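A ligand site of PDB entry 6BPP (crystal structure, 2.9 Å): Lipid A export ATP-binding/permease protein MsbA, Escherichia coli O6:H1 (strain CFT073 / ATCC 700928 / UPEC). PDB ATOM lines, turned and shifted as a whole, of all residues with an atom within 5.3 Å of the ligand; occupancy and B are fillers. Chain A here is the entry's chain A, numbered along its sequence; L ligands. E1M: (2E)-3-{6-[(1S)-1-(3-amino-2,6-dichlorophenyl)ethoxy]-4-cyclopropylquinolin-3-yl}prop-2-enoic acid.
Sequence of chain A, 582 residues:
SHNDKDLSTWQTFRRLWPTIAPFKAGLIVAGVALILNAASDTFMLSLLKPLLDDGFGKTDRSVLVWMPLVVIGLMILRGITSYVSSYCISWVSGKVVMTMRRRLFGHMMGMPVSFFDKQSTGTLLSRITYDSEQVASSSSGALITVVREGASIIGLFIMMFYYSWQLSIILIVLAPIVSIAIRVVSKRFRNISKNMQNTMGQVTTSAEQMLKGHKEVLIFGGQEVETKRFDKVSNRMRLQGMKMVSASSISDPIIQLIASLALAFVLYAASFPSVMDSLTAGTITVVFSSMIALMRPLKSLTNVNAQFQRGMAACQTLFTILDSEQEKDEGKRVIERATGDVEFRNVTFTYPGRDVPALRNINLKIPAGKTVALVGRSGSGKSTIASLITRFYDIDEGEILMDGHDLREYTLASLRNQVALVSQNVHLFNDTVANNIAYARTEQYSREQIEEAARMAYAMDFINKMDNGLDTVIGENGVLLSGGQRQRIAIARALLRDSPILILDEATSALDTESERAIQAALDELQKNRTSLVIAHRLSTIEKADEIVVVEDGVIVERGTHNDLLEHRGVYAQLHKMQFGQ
OG1 of Thr 302 is in hydrogen-bond range of O of Leu 298, at 3.4 Å. The side-chain hydroxyl of Thr 302 is in hydrogen-bond range of the backbone carbonyl oxygen of Lys 299, 3.0 Å away. The side-chain hydroxyl (OG) of Ser 179 lies within hydrogen-bond range of the backbone carbonyl oxygen (O) of Ala 175.
CZ of Phe 157 touches CL12 of the ligand, 3.96 Å away. Leu 171 touches the ligand (O to C1, 3.1 Å). Leu 174 touches the ligand. Ala 175 touches the ligand (CA to O13, 3.2 Å). Val 178 touches the ligand (CG1 to C19, 3.6 Å). Ser 179 touches the ligand. CD1 of Ile 182 touches C20 of the ligand (3.2 Å). Ile 255 touches the ligand (CG2 to C26, 3.7 Å). Ala 259 touches the ligand. Leu 263 touches the ligand. Leu 294 touches the ligand (CD1 to C6, 3.5 Å). Met 295 touches the ligand. Leu 298 touches the ligand (CD1 to C6, 3.7 Å). Hydrophobic or aromatic side chains within 4 Å of the ligand: Phe 157, Leu 171, Leu 174, Ala 175, Val 178, Ile 182, Ile 255, Ala 259, Leu 263, Leu 294, Met 295 and Leu 298. Of the 23 residues printed, 16 come within 4 Å of the ligand.
The backbone carbonyl oxygen (O) of Met 291 sits at hydrogen-bond distance from a nitrogen (N11) of the ligand, at 3.1 Å. An oxygen (O27) of the ligand lies within salt-bridge range of the side-chain amino group of Lys 299 (3.6 Å). NH2 of Arg 190 lies within salt-bridge range of O28 of the ligand (3.3 Å).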
ATOM      1  N   PHE A 157       9.572  33.634  32.696  1.00  0.00           N
ATOM      2  CA  PHE A 157       8.976  32.608  31.856  1.00  0.00           C
ATOM      3  C   PHE A 157       7.452  32.708  31.851  1.00  0.00           C
ATOM      4  O   PHE A 157       6.821  32.504  30.806  1.00  0.00           O
ATOM      5  CB  PHE A 157       9.421  31.208  32.324  1.00  0.00           C
ATOM      6  CG  PHE A 157      10.591  30.642  31.545  1.00  0.00           C
ATOM      7  CD1 PHE A 157      10.666  30.797  30.175  1.00  0.00           C
ATOM      8  CD2 PHE A 157      11.588  29.943  32.202  1.00  0.00           C
ATOM      9  CE1 PHE A 157      11.732  30.276  29.456  1.00  0.00           C
ATOM     10  CE2 PHE A 157      12.660  29.408  31.492  1.00  0.00           C
ATOM     11  CZ  PHE A 157      12.728  29.577  30.113  1.00  0.00           C
ATOM     12  N   LEU A 171      11.361  27.973  22.717  1.00  0.00           N
ATOM     13  CA  LEU A 171      12.571  28.081  23.514  1.00  0.00           C
ATOM     14  C   LEU A 171      12.733  26.889  24.437  1.00  0.00           C
ATOM     15  O   LEU A 171      13.850  26.428  24.665  1.00  0.00           O
ATOM     16  CB  LEU A 171      12.530  29.394  24.309  1.00  0.00           C
ATOM     17  CG  LEU A 171      13.883  30.039  24.595  1.00  0.00           C
ATOM     18  CD1 LEU A 171      14.557  30.525  23.312  1.00  0.00           C
ATOM     19  CD2 LEU A 171      13.650  31.182  25.543  1.00  0.00           C
ATOM     20  N   ILE A 172      11.619  26.382  24.987  1.00  0.00           N
ATOM     21  CA  ILE A 172      11.685  25.216  25.855  1.00  0.00           C
ATOM     22  C   ILE A 172      12.388  24.073  25.140  1.00  0.00           C
ATOM     23  O   ILE A 172      13.471  23.640  25.546  1.00  0.00           O
ATOM     24  CB  ILE A 172      10.273  24.806  26.320  1.00  0.00           C
ATOM     25  CG1 ILE A 172       9.660  25.889  27.209  1.00  0.00           C
ATOM     26  CG2 ILE A 172      10.332  23.474  27.090  1.00  0.00           C
ATOM     27  CD1 ILE A 172       8.205  25.647  27.578  1.00  0.00           C
ATOM     28  N   LEU A 174      14.118  23.795  22.630  1.00  0.00           N
ATOM     29  CA  LEU A 174      15.515  24.109  22.358  1.00  0.00           C
ATOM     30  C   LEU A 174      16.341  24.076  23.636  1.00  0.00           C
ATOM     31  O   LEU A 174      17.519  23.699  23.613  1.00  0.00           O
ATOM     32  CB  LEU A 174      15.621  25.471  21.688  1.00  0.00           C
ATOM     33  CG  LEU A 174      15.231  25.526  20.205  1.00  0.00           C
ATOM     34  CD1 LEU A 174      15.406  26.927  19.650  1.00  0.00           C
ATOM     35  CD2 LEU A 174      16.029  24.531  19.377  1.00  0.00           C
ATOM     36  N   ALA A 175      15.749  24.451  24.768  1.00  0.00           N
ATOM     37  CA  ALA A 175      16.524  24.574  26.008  1.00  0.00           C
ATOM     38  C   ALA A 175      17.338  23.328  26.321  1.00  0.00           C
ATOM     39  O   ALA A 175      18.554  23.459  26.535  1.00  0.00           O
ATOM     40  CB  ALA A 175      15.584  24.957  27.152  1.00  0.00           C
ATOM     41  N   PRO A 176      16.777  22.110  26.359  1.00  0.00           N
ATOM     42  CA  PRO A 176      17.639  20.947  26.617  1.00  0.00           C
ATOM     43  C   PRO A 176      18.831  20.792  25.665  1.00  0.00           C
ATOM     44  O   PRO A 176      19.959  20.681  26.151  1.00  0.00           O
ATOM     45  CB  PRO A 176      16.657  19.780  26.536  1.00  0.00           C
ATOM     46  CG  PRO A 176      15.410  20.367  27.074  1.00  0.00           C
ATOM     47  CD  PRO A 176      15.364  21.771  26.560  1.00  0.00           C
ATOM     48  N   VAL A 178      20.326  22.915  23.961  1.00  0.00           N
ATOM     49  CA  VAL A 178      21.229  24.010  24.291  1.00  0.00           C
ATOM     50  C   VAL A 178      21.996  23.701  25.568  1.00  0.00           C
ATOM     51  O   VAL A 178      23.235  23.810  25.614  1.00  0.00           O
ATOM     52  CB  VAL A 178      20.457  25.337  24.403  1.00  0.00           C
ATOM     53  CG1 VAL A 178      21.388  26.440  24.902  1.00  0.00           C
ATOM     54  CG2 VAL A 178      19.867  25.730  23.060  1.00  0.00           C
ATOM     55  N   SER A 179      21.283  23.323  26.633  1.00  0.00           N
ATOM     56  CA  SER A 179      21.922  23.099  27.922  1.00  0.00           C
ATOM     57  C   SER A 179      23.059  22.089  27.792  1.00  0.00           C
ATOM     58  O   SER A 179      24.166  22.326  28.268  1.00  0.00           O
ATOM     59  CB  SER A 179      20.898  22.606  28.953  1.00  0.00           C
ATOM     60  OG  SER A 179      19.866  23.550  29.160  1.00  0.00           O
ATOM     61  N   ILE A 182      25.952  23.619  25.910  1.00  0.00           N
ATOM     62  CA  ILE A 182      26.658  24.539  26.792  1.00  0.00           C
ATOM     63  C   ILE A 182      27.454  23.771  27.837  1.00  0.00           C
ATOM     64  O   ILE A 182      28.642  24.044  28.074  1.00  0.00           O
ATOM     65  CB  ILE A 182      25.674  25.520  27.453  1.00  0.00           C
ATOM     66  CG1 ILE A 182      25.029  26.411  26.380  1.00  0.00           C
ATOM     67  CG2 ILE A 182      26.372  26.369  28.517  1.00  0.00           C
ATOM     68  CD1 ILE A 182      23.921  27.288  26.905  1.00  0.00           C
ATOM     69  N   ARG A 190      36.954  24.902  30.731  1.00  0.00           N
ATOM     70  CA  ARG A 190      37.222  25.705  31.927  1.00  0.00           C
ATOM     71  C   ARG A 190      36.888  24.916  33.185  1.00  0.00           C
ATOM     72  O   ARG A 190      35.824  25.092  33.796  1.00  0.00           O
ATOM     73  CB  ARG A 190      36.444  26.989  31.842  1.00  0.00           C
ATOM     74  CG  ARG A 190      34.966  26.796  31.674  1.00  0.00           C
ATOM     75  CD  ARG A 190      34.256  28.110  31.702  1.00  0.00           C
ATOM     76  NE  ARG A 190      32.816  27.911  31.656  1.00  0.00           N
ATOM     77  CZ  ARG A 190      31.924  28.893  31.643  1.00  0.00           C
ATOM     78  NH1 ARG A 190      32.327  30.156  31.671  1.00  0.00           N
ATOM     79  NH2 ARG A 190      30.628  28.603  31.599  1.00  0.00           N
ATOM     80  N   ILE A 255      29.460  29.682  23.883  1.00  0.00           N
ATOM     81  CA  ILE A 255      28.226  29.499  24.661  1.00  0.00           C
ATOM     82  C   ILE A 255      27.201  30.535  24.244  1.00  0.00           C
ATOM     83  O   ILE A 255      26.019  30.218  24.038  1.00  0.00           O
ATOM     84  CB  ILE A 255      28.521  29.557  26.167  1.00  0.00           C
ATOM     85  CG1 ILE A 255      29.359  28.349  26.602  1.00  0.00           C
ATOM     86  CG2 ILE A 255      27.207  29.584  26.963  1.00  0.00           C
ATOM     87  CD1 ILE A 255      29.811  28.378  28.058  1.00  0.00           C
ATOM     88  N   ALA A 259      23.352  29.873  22.438  1.00  0.00           N
ATOM     89  CA  ALA A 259      22.106  30.498  22.878  1.00  0.00           C
ATOM     90  C   ALA A 259      21.560  31.437  21.812  1.00  0.00           C
ATOM     91  O   ALA A 259      20.343  31.530  21.603  1.00  0.00           O
ATOM     92  CB  ALA A 259      22.345  31.255  24.193  1.00  0.00           C
ATOM     93  N   SER A 260      22.461  32.149  21.113  1.00  0.00           N
ATOM     94  CA  SER A 260      22.028  33.096  20.098  1.00  0.00           C
ATOM     95  C   SER A 260      21.349  32.386  18.924  1.00  0.00           C
ATOM     96  O   SER A 260      20.405  32.927  18.337  1.00  0.00           O
ATOM     97  CB  SER A 260      23.223  33.912  19.602  1.00  0.00           C
ATOM     98  OG  SER A 260      22.828  34.773  18.556  1.00  0.00           O
ATOM     99  N   ALA A 262      19.607  29.513  19.045  1.00  0.00           N
ATOM    100  CA  ALA A 262      18.262  29.244  19.530  1.00  0.00           C
ATOM    101  C   ALA A 262      17.378  30.478  19.391  1.00  0.00           C
ATOM    102  O   ALA A 262      16.272  30.409  18.845  1.00  0.00           O
ATOM    103  CB  ALA A 262      18.329  28.782  20.988  1.00  0.00           C
ATOM    104  N   LEU A 263      17.854  31.620  19.889  1.00  0.00           N
ATOM    105  CA  LEU A 263      17.093  32.858  19.759  1.00  0.00           C
ATOM    106  C   LEU A 263      16.808  33.179  18.299  1.00  0.00           C
ATOM    107  O   LEU A 263      15.664  33.489  17.939  1.00  0.00           O
ATOM    108  CB  LEU A 263      17.848  34.008  20.430  1.00  0.00           C
ATOM    109  CG  LEU A 263      17.793  34.081  21.960  1.00  0.00           C
ATOM    110  CD1 LEU A 263      18.565  35.291  22.448  1.00  0.00           C
ATOM    111  CD2 LEU A 263      16.355  34.141  22.461  1.00  0.00           C
ATOM    112  N   MET A 291      13.693  37.130  27.029  1.00  0.00           N
ATOM    113  CA  MET A 291      14.621  36.066  26.642  1.00  0.00           C
ATOM    114  C   MET A 291      16.057  36.507  26.867  1.00  0.00           C
ATOM    115  O   MET A 291      16.885  35.733  27.373  1.00  0.00           O
ATOM    116  CB  MET A 291      14.402  35.676  25.182  1.00  0.00           C
ATOM    117  CG  MET A 291      13.157  34.837  24.970  1.00  0.00           C
ATOM    118  SD  MET A 291      12.745  34.549  23.238  1.00  0.00           S
ATOM    119  CE  MET A 291      11.142  33.764  23.443  1.00  0.00           C
ATOM    120  N   ILE A 292      16.377  37.744  26.500  1.00  0.00           N
ATOM    121  CA  ILE A 292      17.732  38.266  26.717  1.00  0.00           C
ATOM    122  C   ILE A 292      18.009  38.394  28.210  1.00  0.00           C
ATOM    123  O   ILE A 292      19.139  38.148  28.657  1.00  0.00           O
ATOM    124  CB  ILE A 292      17.887  39.620  25.982  1.00  0.00           C
ATOM    125  CG1 ILE A 292      17.910  39.368  24.474  1.00  0.00           C
ATOM    126  CG2 ILE A 292      19.162  40.341  26.439  1.00  0.00           C
ATOM    127  CD1 ILE A 292      17.818  40.623  23.632  1.00  0.00           C
ATOM    128  N   LEU A 294      16.884  36.409  30.547  1.00  0.00           N
ATOM    129  CA  LEU A 294      17.071  35.076  31.112  1.00  0.00           C
ATOM    130  C   LEU A 294      18.522  34.627  31.085  1.00  0.00           C
ATOM    131  O   LEU A 294      18.946  33.880  31.971  1.00  0.00           O
ATOM    132  CB  LEU A 294      16.219  34.066  30.339  1.00  0.00           C
ATOM    133  CG  LEU A 294      14.723  34.035  30.696  1.00  0.00           C
ATOM    134  CD1 LEU A 294      13.990  33.156  29.709  1.00  0.00           C
ATOM    135  CD2 LEU A 294      14.535  33.543  32.115  1.00  0.00           C
ATOM    136  N   MET A 295      19.297  35.060  30.094  1.00  0.00           N
ATOM    137  CA  MET A 295      20.639  34.512  29.915  1.00  0.00           C
ATOM    138  C   MET A 295      21.479  34.671  31.168  1.00  0.00           C
ATOM    139  O   MET A 295      22.205  33.754  31.554  1.00  0.00           O
ATOM    140  CB  MET A 295      21.304  35.160  28.712  1.00  0.00           C
ATOM    141  CG  MET A 295      20.571  34.921  27.408  1.00  0.00           C
ATOM    142  SD  MET A 295      21.525  35.439  25.960  1.00  0.00           S
ATOM    143  CE  MET A 295      21.606  37.197  26.236  1.00  0.00           C
ATOM    144  N   LEU A 298      20.321  32.110  34.048  1.00  0.00           N
ATOM    145  CA  LEU A 298      20.629  30.721  33.727  1.00  0.00           C
ATOM    146  C   LEU A 298      22.109  30.430  33.869  1.00  0.00           C
ATOM    147  O   LEU A 298      22.508  29.355  34.333  1.00  0.00           O
ATOM    148  CB  LEU A 298      20.157  30.399  32.309  1.00  0.00           C
ATOM    149  CG  LEU A 298      18.649  30.512  32.101  1.00  0.00           C
ATOM    150  CD1 LEU A 298      18.285  30.327  30.626  1.00  0.00           C
ATOM    151  CD2 LEU A 298      17.899  29.503  32.972  1.00  0.00           C
ATOM    152  N   LYS A 299      22.952  31.374  33.462  1.00  0.00           N
ATOM    153  CA  LYS A 299      24.386  31.226  33.655  1.00  0.00           C
ATOM    154  C   LYS A 299      24.728  31.029  35.124  1.00  0.00           C
ATOM    155  O   LYS A 299      25.466  30.105  35.500  1.00  0.00           O
ATOM    156  CB  LYS A 299      25.113  32.441  33.089  1.00  0.00           C
ATOM    157  CG  LYS A 299      26.583  32.482  33.398  1.00  0.00           C
ATOM    158  CD  LYS A 299      27.274  33.556  32.588  1.00  0.00           C
ATOM    159  CE  LYS A 299      28.776  33.506  32.772  1.00  0.00           C
ATOM    160  NZ  LYS A 299      29.427  32.767  31.657  1.00  0.00           N
ATOM    161  N   THR A 302      23.613  27.339  36.765  1.00  0.00           N
ATOM    162  CA  THR A 302      24.452  26.193  36.430  1.00  0.00           C
ATOM    163  C   THR A 302      25.797  26.268  37.136  1.00  0.00           C
ATOM    164  O   THR A 302      26.374  25.233  37.506  1.00  0.00           O
ATOM    165  CB  THR A 302      24.637  26.110  34.916  1.00  0.00           C
ATOM    166  OG1 THR A 302      25.222  27.333  34.452  1.00  0.00           O
ATOM    167  CG2 THR A 302      23.286  25.907  34.239  1.00  0.00           C
ATOM    168  N   ASN A 303      26.319  27.476  37.349  1.00  0.00           N
ATOM    169  CA  ASN A 303      27.608  27.656  38.009  1.00  0.00           C
ATOM    170  C   ASN A 303      27.552  27.550  39.528  1.00  0.00           C
ATOM    171  O   ASN A 303      28.608  27.521  40.166  1.00  0.00           O
ATOM    172  CB  ASN A 303      28.228  29.012  37.640  1.00  0.00           C
ATOM    173  CG  ASN A 303      28.710  29.064  36.219  1.00  0.00           C
ATOM    174  OD1 ASN A 303      28.711  28.064  35.507  1.00  0.00           O
ATOM    175  ND2 ASN A 303      29.137  30.251  35.779  1.00  0.00           N
HETATM  176  C4  E1M L   1      17.332  29.750  26.180  1.00  0.00           C
HETATM  177  C14 E1M L   1      18.921  27.461  27.473  1.00  0.00           C
HETATM  178  C5  E1M L   1      16.392  29.809  27.191  1.00  0.00           C
HETATM  179  C6  E1M L   1      16.053  31.027  27.762  1.00  0.00           C
HETATM  180  C7  E1M L   1      16.647  32.199  27.315  1.00  0.00           C
HETATM  181  C8  E1M L   1      17.590  32.153  26.300  1.00  0.00           C
HETATM  182  C9  E1M L   1      17.926  30.922  25.733  1.00  0.00           C
HETATM  183  C1  E1M L   1      16.593  27.947  24.619  1.00  0.00           C
HETATM  184  C15 E1M L   1      18.879  26.437  28.426  1.00  0.00           C
HETATM  185  C16 E1M L   1      19.824  26.338  29.393  1.00  0.00           C
HETATM  186  C17 E1M L   1      20.879  27.261  29.462  1.00  0.00           C
HETATM  187  C18 E1M L   1      20.947  28.308  28.503  1.00  0.00           C
HETATM  188  C19 E1M L   1      19.934  28.389  27.507  1.00  0.00           C
HETATM  189  C2  E1M L   1      17.714  28.416  25.545  1.00  0.00           C
HETATM  190  C20 E1M L   1      22.015  29.222  28.596  1.00  0.00           C
HETATM  191  C21 E1M L   1      22.960  29.023  29.626  1.00  0.00           C
HETATM  192  C22 E1M L   1      22.810  27.949  30.524  1.00  0.00           C
HETATM  193  C24 E1M L   1      24.118  29.905  29.792  1.00  0.00           C
HETATM  194  C25 E1M L   1      25.223  29.425  30.399  1.00  0.00           C
HETATM  195  C26 E1M L   1      26.415  30.251  30.566  1.00  0.00           C
HETATM  196  C29 E1M L   1      22.163  30.358  27.620  1.00  0.00           C
HETATM  197  C30 E1M L   1      21.012  31.347  27.446  1.00  0.00           C
HETATM  198  C31 E1M L   1      22.248  31.760  28.232  1.00  0.00           C
HETATM  199  N11 E1M L   1      18.185  33.353  25.863  1.00  0.00           N
HETATM  200  N23 E1M L   1      21.798  27.131  30.430  1.00  0.00           N
HETATM  201  O13 E1M L   1      17.902  27.426  26.554  1.00  0.00           O
HETATM  202  O27 E1M L   1      26.437  31.394  30.166  1.00  0.00           O
HETATM  203  O28 E1M L   1      27.500  29.725  31.183  1.00  0.00           O
HETATM  204 CL10 E1M L   1      19.099  30.790  24.448  1.00  0.00          CL
HETATM  205 CL12 E1M L   1      15.652  28.332  27.743  1.00  0.00          CL
